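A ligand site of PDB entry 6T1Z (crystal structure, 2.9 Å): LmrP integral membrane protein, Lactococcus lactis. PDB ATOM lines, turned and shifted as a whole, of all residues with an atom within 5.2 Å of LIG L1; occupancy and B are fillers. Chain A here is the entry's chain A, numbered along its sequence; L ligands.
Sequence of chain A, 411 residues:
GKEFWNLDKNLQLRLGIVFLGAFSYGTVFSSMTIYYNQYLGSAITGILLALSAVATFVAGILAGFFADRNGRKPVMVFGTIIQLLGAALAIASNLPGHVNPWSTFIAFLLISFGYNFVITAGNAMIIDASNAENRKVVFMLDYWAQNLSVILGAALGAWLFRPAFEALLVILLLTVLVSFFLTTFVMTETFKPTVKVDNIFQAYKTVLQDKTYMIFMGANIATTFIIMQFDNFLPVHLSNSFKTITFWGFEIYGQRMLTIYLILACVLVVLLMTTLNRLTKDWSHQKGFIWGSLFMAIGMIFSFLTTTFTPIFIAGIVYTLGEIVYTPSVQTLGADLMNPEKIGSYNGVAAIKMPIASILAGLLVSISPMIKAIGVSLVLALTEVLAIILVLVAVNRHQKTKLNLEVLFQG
OE1 of Glu 323 is in salt-bridge range of N6 of LIG L1 (2.8 Å). The side-chain carboxylate (OD1) of Asp 231 lies close to a nitrogen (N4) of LIG L1 (2.9 Å).
OE2 of Glu 323 is in hydrogen-bond range of OH of Tyr 319 (2.6 Å). The side-chain carboxylate (OE1) of Glu 323 is in hydrogen-bond range of the side-chain hydroxyl (OH) of Tyr 143, at 2.6 Å. O of Leu 262 sits at hydrogen-bond distance from SG of Cys 266 (3.3 Å). The backbone carbonyl oxygen (O) of Tyr 143 lies within hydrogen-bond range of the side-chain amide nitrogen (ND2) of Asn 147 (2.8 Å).
Ala 53 touches LIG L1. CG2 of Val 54 touches C27 of LIG L1, at 3.7 Å. Asn 147 touches LIG L1 (OD1 to C25, 3.2 Å). Ile 227 touches LIG L1 (CG2 to C20, 3.8 Å). Met 228 touches LIG L1. CB of Phe 230 touches C17 of LIG L1, 3.8 Å away. C of Ala 265 touches C25 of LIG L1 (3.6 Å). Cys 266 touches LIG L1. Met 354 touches LIG L1. Pro 355 touches LIG L1. Ser 358 touches LIG L1. Hydrophobic or aromatic side chains within 4 Å of LIG L1: Ala 53, Val 54, Ile 227, Met 228, Phe 230, Ala 265, Met 354 and Pro 355. The nearest printed residue that does not touch LIG L1 is Val 269 (4.1 Å).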
ATOM      1  N   ALA A  50      -0.259 -31.470 -28.208  1.00  0.00           N
ATOM      2  CA  ALA A  50      -0.713 -30.304 -28.956  1.00  0.00           C
ATOM      3  C   ALA A  50      -2.156 -30.045 -28.612  1.00  0.00           C
ATOM      4  O   ALA A  50      -2.486 -28.907 -28.272  1.00  0.00           O
ATOM      5  CB  ALA A  50      -0.578 -30.560 -30.441  1.00  0.00           C
ATOM      6  N   ALA A  53      -2.627 -28.717 -24.935  1.00  0.00           N
ATOM      7  CA  ALA A  53      -2.196 -27.319 -24.871  1.00  0.00           C
ATOM      8  C   ALA A  53      -3.274 -26.364 -25.404  1.00  0.00           C
ATOM      9  O   ALA A  53      -3.526 -25.324 -24.785  1.00  0.00           O
ATOM     10  CB  ALA A  53      -0.900 -27.149 -25.639  1.00  0.00           C
ATOM     11  N   VAL A  54      -3.909 -26.739 -26.548  1.00  0.00           N
ATOM     12  CA  VAL A  54      -5.015 -25.992 -27.179  1.00  0.00           C
ATOM     13  C   VAL A  54      -6.227 -26.069 -26.240  1.00  0.00           C
ATOM     14  O   VAL A  54      -6.886 -25.058 -25.991  1.00  0.00           O
ATOM     15  CB  VAL A  54      -5.368 -26.557 -28.578  1.00  0.00           C
ATOM     16  CG1 VAL A  54      -6.672 -25.952 -29.106  1.00  0.00           C
ATOM     17  CG2 VAL A  54      -4.246 -26.345 -29.571  1.00  0.00           C
ATOM     18  N   TYR A 143       4.627 -18.300  -6.519  1.00  0.00           N
ATOM     19  CA  TYR A 143       5.769 -18.727  -7.309  1.00  0.00           C
ATOM     20  C   TYR A 143       6.744 -19.625  -6.550  1.00  0.00           C
ATOM     21  O   TYR A 143       7.263 -20.571  -7.112  1.00  0.00           O
ATOM     22  CB  TYR A 143       6.470 -17.465  -7.839  1.00  0.00           C
ATOM     23  CG  TYR A 143       7.745 -17.699  -8.604  1.00  0.00           C
ATOM     24  CD1 TYR A 143       7.736 -18.321  -9.845  1.00  0.00           C
ATOM     25  CD2 TYR A 143       8.963 -17.262  -8.099  1.00  0.00           C
ATOM     26  CE1 TYR A 143       8.914 -18.524 -10.560  1.00  0.00           C
ATOM     27  CE2 TYR A 143      10.148 -17.468  -8.796  1.00  0.00           C
ATOM     28  CZ  TYR A 143      10.112 -18.100 -10.026  1.00  0.00           C
ATOM     29  OH  TYR A 143      11.265 -18.314 -10.721  1.00  0.00           O
ATOM     30  N   ASN A 147       7.438 -24.013  -6.982  1.00  0.00           N
ATOM     31  CA  ASN A 147       8.789 -24.527  -7.193  1.00  0.00           C
ATOM     32  C   ASN A 147       9.168 -25.583  -6.165  1.00  0.00           C
ATOM     33  O   ASN A 147       9.610 -26.668  -6.556  1.00  0.00           O
ATOM     34  CB  ASN A 147       9.798 -23.371  -7.247  1.00  0.00           C
ATOM     35  CG  ASN A 147       9.847 -22.650  -8.569  1.00  0.00           C
ATOM     36  OD1 ASN A 147      10.872 -22.617  -9.256  1.00  0.00           O
ATOM     37  ND2 ASN A 147       8.752 -22.017  -8.973  1.00  0.00           N
ATOM     38  N   ILE A 227      12.038 -17.770 -21.394  1.00  0.00           N
ATOM     39  CA  ILE A 227      11.694 -18.959 -20.595  1.00  0.00           C
ATOM     40  C   ILE A 227      11.382 -20.137 -21.526  1.00  0.00           C
ATOM     41  O   ILE A 227      11.777 -21.258 -21.212  1.00  0.00           O
ATOM     42  CB  ILE A 227      10.538 -18.690 -19.597  1.00  0.00           C
ATOM     43  CG1 ILE A 227      10.932 -17.606 -18.578  1.00  0.00           C
ATOM     44  CG2 ILE A 227      10.088 -20.019 -18.903  1.00  0.00           C
ATOM     45  CD1 ILE A 227       9.870 -17.098 -17.751  1.00  0.00           C
ATOM     46  N   MET A 228      10.722 -19.864 -22.690  1.00  0.00           N
ATOM     47  CA  MET A 228      10.353 -20.835 -23.731  1.00  0.00           C
ATOM     48  C   MET A 228      11.555 -21.464 -24.390  1.00  0.00           C
ATOM     49  O   MET A 228      11.413 -22.345 -25.256  1.00  0.00           O
ATOM     50  CB  MET A 228       9.428 -20.208 -24.781  1.00  0.00           C
ATOM     51  CG  MET A 228       8.040 -19.916 -24.255  1.00  0.00           C
ATOM     52  SD  MET A 228       7.365 -21.158 -23.152  1.00  0.00           S
ATOM     53  CE  MET A 228       7.643 -20.386 -21.621  1.00  0.00           C
ATOM     54  N   PHE A 230      13.860 -23.341 -22.734  1.00  0.00           N
ATOM     55  CA  PHE A 230      13.919 -24.705 -22.175  1.00  0.00           C
ATOM     56  C   PHE A 230      13.083 -25.697 -22.989  1.00  0.00           C
ATOM     57  O   PHE A 230      13.431 -26.871 -23.099  1.00  0.00           O
ATOM     58  CB  PHE A 230      13.386 -24.709 -20.744  1.00  0.00           C
ATOM     59  CG  PHE A 230      14.251 -24.013 -19.748  1.00  0.00           C
ATOM     60  CD1 PHE A 230      14.178 -22.636 -19.585  1.00  0.00           C
ATOM     61  CD2 PHE A 230      15.121 -24.727 -18.926  1.00  0.00           C
ATOM     62  CE1 PHE A 230      14.945 -21.988 -18.611  1.00  0.00           C
ATOM     63  CE2 PHE A 230      15.876 -24.082 -17.958  1.00  0.00           C
ATOM     64  CZ  PHE A 230      15.800 -22.710 -17.817  1.00  0.00           C
ATOM     65  N   ASP A 231      11.948 -25.217 -23.518  1.00  0.00           N
ATOM     66  CA  ASP A 231      11.013 -25.960 -24.347  1.00  0.00           C
ATOM     67  C   ASP A 231      11.496 -26.168 -25.789  1.00  0.00           C
ATOM     68  O   ASP A 231      11.196 -27.235 -26.356  1.00  0.00           O
ATOM     69  CB  ASP A 231       9.680 -25.207 -24.430  1.00  0.00           C
ATOM     70  CG  ASP A 231       8.773 -25.449 -23.260  1.00  0.00           C
ATOM     71  OD1 ASP A 231       9.282 -25.718 -22.161  1.00  0.00           O
ATOM     72  OD2 ASP A 231       7.533 -25.383 -23.449  1.00  0.00           O
ATOM     73  N   LEU A 262      17.121 -27.596 -14.853  1.00  0.00           N
ATOM     74  CA  LEU A 262      15.778 -27.442 -14.298  1.00  0.00           C
ATOM     75  C   LEU A 262      15.801 -27.631 -12.786  1.00  0.00           C
ATOM     76  O   LEU A 262      15.322 -26.763 -12.067  1.00  0.00           O
ATOM     77  CB  LEU A 262      14.782 -28.434 -14.917  1.00  0.00           C
ATOM     78  CG  LEU A 262      14.314 -28.170 -16.325  1.00  0.00           C
ATOM     79  CD1 LEU A 262      13.330 -29.228 -16.763  1.00  0.00           C
ATOM     80  CD2 LEU A 262      13.659 -26.808 -16.440  1.00  0.00           C
ATOM     81  N   ALA A 265      17.717 -24.733 -11.078  1.00  0.00           N
ATOM     82  CA  ALA A 265      16.888 -23.537 -11.116  1.00  0.00           C
ATOM     83  C   ALA A 265      15.772 -23.550 -10.083  1.00  0.00           C
ATOM     84  O   ALA A 265      15.670 -22.598  -9.304  1.00  0.00           O
ATOM     85  CB  ALA A 265      16.317 -23.323 -12.521  1.00  0.00           C
ATOM     86  N   CYS A 266      14.979 -24.632 -10.020  1.00  0.00           N
ATOM     87  CA  CYS A 266      13.921 -24.756  -9.025  1.00  0.00           C
ATOM     88  C   CYS A 266      14.509 -24.691  -7.603  1.00  0.00           C
ATOM     89  O   CYS A 266      14.003 -23.937  -6.783  1.00  0.00           O
ATOM     90  CB  CYS A 266      13.100 -26.034  -9.247  1.00  0.00           C
ATOM     91  SG  CYS A 266      12.281 -26.136 -10.854  1.00  0.00           S
ATOM     92  N   VAL A 269      15.518 -21.117  -6.763  1.00  0.00           N
ATOM     93  CA  VAL A 269      14.316 -20.328  -6.440  1.00  0.00           C
ATOM     94  C   VAL A 269      13.899 -20.586  -4.991  1.00  0.00           C
ATOM     95  O   VAL A 269      13.728 -19.638  -4.237  1.00  0.00           O
ATOM     96  CB  VAL A 269      13.160 -20.610  -7.431  1.00  0.00           C
ATOM     97  CG1 VAL A 269      11.818 -20.172  -6.861  1.00  0.00           C
ATOM     98  CG2 VAL A 269      13.399 -19.949  -8.783  1.00  0.00           C
ATOM     99  N   TYR A 319      20.701 -16.928 -14.882  1.00  0.00           N
ATOM    100  CA  TYR A 319      19.330 -16.952 -15.389  1.00  0.00           C
ATOM    101  C   TYR A 319      18.355 -17.023 -14.241  1.00  0.00           C
ATOM    102  O   TYR A 319      17.406 -16.245 -14.212  1.00  0.00           O
ATOM    103  CB  TYR A 319      19.100 -18.115 -16.353  1.00  0.00           C
ATOM    104  CG  TYR A 319      17.633 -18.352 -16.638  1.00  0.00           C
ATOM    105  CD1 TYR A 319      16.985 -17.701 -17.684  1.00  0.00           C
ATOM    106  CD2 TYR A 319      16.872 -19.200 -15.838  1.00  0.00           C
ATOM    107  CE1 TYR A 319      15.633 -17.887 -17.931  1.00  0.00           C
ATOM    108  CE2 TYR A 319      15.513 -19.366 -16.056  1.00  0.00           C
ATOM    109  CZ  TYR A 319      14.902 -18.715 -17.107  1.00  0.00           C
ATOM    110  OH  TYR A 319      13.577 -18.937 -17.352  1.00  0.00           O
ATOM    111  N   GLU A 323      15.226 -14.662 -13.319  1.00  0.00           N
ATOM    112  CA  GLU A 323      13.882 -15.193 -13.229  1.00  0.00           C
ATOM    113  C   GLU A 323      13.211 -14.888 -11.883  1.00  0.00           C
ATOM    114  O   GLU A 323      12.076 -14.412 -11.901  1.00  0.00           O
ATOM    115  CB  GLU A 323      13.848 -16.681 -13.557  1.00  0.00           C
ATOM    116  CG  GLU A 323      12.462 -17.279 -13.563  1.00  0.00           C
ATOM    117  CD  GLU A 323      12.458 -18.779 -13.773  1.00  0.00           C
ATOM    118  OE1 GLU A 323      12.358 -19.532 -12.792  1.00  0.00           O
ATOM    119  OE2 GLU A 323      12.552 -19.199 -14.940  1.00  0.00           O
ATOM    120  N   MET A 354       2.093 -17.595 -23.294  1.00  0.00           N
ATOM    121  CA  MET A 354       2.802 -18.875 -23.310  1.00  0.00           C
ATOM    122  C   MET A 354       2.755 -19.548 -24.678  1.00  0.00           C
ATOM    123  O   MET A 354       3.834 -19.886 -25.153  1.00  0.00           O
ATOM    124  CB  MET A 354       2.336 -19.823 -22.194  1.00  0.00           C
ATOM    125  CG  MET A 354       2.604 -19.283 -20.796  1.00  0.00           C
ATOM    126  SD  MET A 354       4.324 -19.563 -20.298  1.00  0.00           S
ATOM    127  CE  MET A 354       4.246 -19.021 -18.599  1.00  0.00           C
ATOM    128  N   PRO A 355       1.580 -19.720 -25.370  1.00  0.00           N
ATOM    129  CA  PRO A 355       1.590 -20.336 -26.707  1.00  0.00           C
ATOM    130  C   PRO A 355       2.390 -19.551 -27.749  1.00  0.00           C
ATOM    131  O   PRO A 355       3.178 -20.156 -28.451  1.00  0.00           O
ATOM    132  CB  PRO A 355       0.110 -20.422 -27.088  1.00  0.00           C
ATOM    133  CG  PRO A 355      -0.568 -19.451 -26.225  1.00  0.00           C
ATOM    134  CD  PRO A 355       0.194 -19.424 -24.955  1.00  0.00           C
ATOM    135  N   SER A 358       6.038 -19.613 -27.087  1.00  0.00           N
ATOM    136  CA  SER A 358       6.457 -20.979 -27.392  1.00  0.00           C
ATOM    137  C   SER A 358       6.561 -21.198 -28.890  1.00  0.00           C
ATOM    138  O   SER A 358       7.598 -21.695 -29.346  1.00  0.00           O
ATOM    139  CB  SER A 358       5.520 -21.995 -26.749  1.00  0.00           C
ATOM    140  OG  SER A 358       5.787 -23.300 -27.241  1.00  0.00           O
ATOM    141  N   ILE A 359       5.517 -20.815 -29.658  1.00  0.00           N
ATOM    142  CA  ILE A 359       5.487 -20.958 -31.114  1.00  0.00           C
ATOM    143  C   ILE A 359       6.669 -20.210 -31.732  1.00  0.00           C
ATOM    144  O   ILE A 359       7.400 -20.792 -32.527  1.00  0.00           O
ATOM    145  CB  ILE A 359       4.130 -20.557 -31.727  1.00  0.00           C
ATOM    146  CG1 ILE A 359       3.063 -21.607 -31.390  1.00  0.00           C
ATOM    147  CG2 ILE A 359       4.248 -20.334 -33.239  1.00  0.00           C
ATOM    148  CD1 ILE A 359       1.688 -21.356 -32.004  1.00  0.00           C
HETATM  149  C1  LIG L   1       0.819 -24.231 -27.976  1.00  0.00           C
HETATM  150  O1  LIG L   1       0.429 -24.545 -29.261  1.00  0.00           O
HETATM  151  C2  LIG L   1       0.045 -23.899 -26.868  1.00  0.00           C
HETATM  152  C3  LIG L   1       0.635 -23.802 -25.618  1.00  0.00           C
HETATM  153  C4  LIG L   1       1.994 -24.023 -25.458  1.00  0.00           C
HETATM  154  C5  LIG L   1       2.774 -24.318 -26.583  1.00  0.00           C
HETATM  155  C6  LIG L   1       2.191 -24.409 -27.836  1.00  0.00           C
HETATM  156  C7  LIG L   1       2.638 -23.968 -24.129  1.00  0.00           C
HETATM  157  N1  LIG L   1       3.979 -24.173 -23.947  1.00  0.00           N
HETATM  158  C8  LIG L   1       4.237 -23.989 -22.608  1.00  0.00           C
HETATM  159  C9  LIG L   1       3.010 -23.681 -22.017  1.00  0.00           C
HETATM  160  N2  LIG L   1       2.009 -23.665 -22.992  1.00  0.00           N
HETATM  161  C10 LIG L   1       2.940 -23.435 -20.640  1.00  0.00           C
HETATM  162  C11 LIG L   1       4.105 -23.486 -19.890  1.00  0.00           C
HETATM  163  C12 LIG L   1       5.347 -23.766 -20.493  1.00  0.00           C
HETATM  164  C13 LIG L   1       5.410 -24.034 -21.860  1.00  0.00           C
HETATM  165  C14 LIG L   1       6.603 -23.724 -19.720  1.00  0.00           C
HETATM  166  N3  LIG L   1       6.712 -23.122 -18.494  1.00  0.00           N
HETATM  167  C15 LIG L   1       8.027 -23.281 -18.068  1.00  0.00           C
HETATM  168  C16 LIG L   1       8.657 -23.976 -19.098  1.00  0.00           C
HETATM  169  N4  LIG L   1       7.750 -24.245 -20.119  1.00  0.00           N
HETATM  170  C17 LIG L   1      10.002 -24.344 -18.963  1.00  0.00           C
HETATM  171  C18 LIG L   1      10.662 -24.042 -17.790  1.00  0.00           C
HETATM  172  C19 LIG L   1      10.028 -23.365 -16.729  1.00  0.00           C
HETATM  173  C20 LIG L   1       8.697 -22.961 -16.897  1.00  0.00           C
HETATM  174  N5  LIG L   1      10.712 -23.138 -15.527  1.00  0.00           N
HETATM  175  C21 LIG L   1       9.954 -22.709 -14.340  1.00  0.00           C
HETATM  176  C22 LIG L   1      10.746 -22.980 -13.067  1.00  0.00           C
HETATM  177  N6  LIG L   1      12.057 -22.343 -13.131  1.00  0.00           N
HETATM  178  C23 LIG L   1      12.809 -22.879 -14.260  1.00  0.00           C
HETATM  179  C24 LIG L   1      12.080 -22.603 -15.571  1.00  0.00           C
HETATM  180  C25 LIG L   1      12.779 -22.545 -11.879  1.00  0.00           C
HETATM  181  C26 LIG L   1      -0.972 -24.547 -29.559  1.00  0.00           C
HETATM  182  C27 LIG L   1      -1.104 -24.924 -30.995  1.00  0.00           C
HETATM  183  O1  LG2 L   2       0.502 -19.703 -17.845  1.00  0.00           O
HETATM  184  O2  LG2 L   2      -0.463 -20.037 -15.497  1.00  0.00           O
HETATM  185  P1  LG2 L   2       0.246 -20.629 -16.696  1.00  0.00           P
HETATM  186  O3  LG2 L   2       1.566 -21.377 -16.295  1.00  0.00           O
HETATM  187  O4  LG2 L   2      -0.717 -21.766 -17.261  1.00  0.00           O
HETATM  188  C1  LG2 L   2      -0.211 -22.695 -18.216  1.00  0.00           C
HETATM  189  C2  LG2 L   2      -0.682 -24.078 -17.858  1.00  0.00           C
HETATM  190  C3  LG2 L   2      -0.983 -24.775 -19.151  1.00  0.00           C
HETATM  191  O5  LG2 L   2      -0.996 -26.224 -19.135  1.00  0.00           O
HETATM  192  C4  LG2 L   2      -0.851 -26.837 -20.309  1.00  0.00           C
HETATM  193  O6  LG2 L   2      -0.348 -26.329 -21.276  1.00  0.00           O
HETATM  194  C5  LG2 L   2      -1.474 -28.212 -20.316  1.00  0.00           C
HETATM  195  C6  LG2 L   2      -0.789 -29.213 -19.415  1.00  0.00           C
HETATM  196  C7  LG2 L   2      -0.613 -28.713 -17.996  1.00  0.00           C
HETATM  197  C8  LG2 L   2      -1.548 -29.359 -17.020  1.00  0.00           C
HETATM  198  C9  LG2 L   2      -1.152 -29.053 -15.605  1.00  0.00           C
HETATM  199  C10 LG2 L   2      -1.873 -29.951 -14.622  1.00  0.00           C
HETATM  200  C11 LG2 L   2      -1.311 -29.857 -13.214  1.00  0.00           C
HETATM  201  C12 LG2 L   2      -1.810 -30.927 -12.254  1.00  0.00           C
HETATM  202  C13 LG2 L   2      -3.169 -30.679 -11.650  1.00  0.00           C
HETATM  203  C14 LG2 L   2      -3.367 -31.478 -10.378  1.00  0.00           C
HETATM  204  C15 LG2 L   2      -4.488 -30.981  -9.471  1.00  0.00           C
HETATM  205  O7  LG2 L   2       0.423 -24.676 -17.117  1.00  0.00           O
HETATM  206  C16 LG2 L   2       0.595 -24.352 -15.810  1.00  0.00           C
HETATM  207  O8  LG2 L   2      -0.263 -23.853 -15.133  1.00  0.00           O
HETATM  208  C17 LG2 L   2       1.987 -24.680 -15.331  1.00  0.00           C
HETATM  209  C18 LG2 L   2       2.140 -26.126 -14.875  1.00  0.00           C
HETATM  210  C19 LG2 L   2       2.601 -26.292 -13.421  1.00  0.00           C
HETATM  211  C20 LG2 L   2       3.934 -25.625 -13.121  1.00  0.00           C
HETATM  212  C21 LG2 L   2       4.742 -26.208 -11.965  1.00  0.00           C
HETATM  213  C22 LG2 L   2       5.932 -25.349 -11.538  1.00  0.00           C
HETATM  214  C23 LG2 L   2       6.683 -24.605 -12.634  1.00  0.00           C
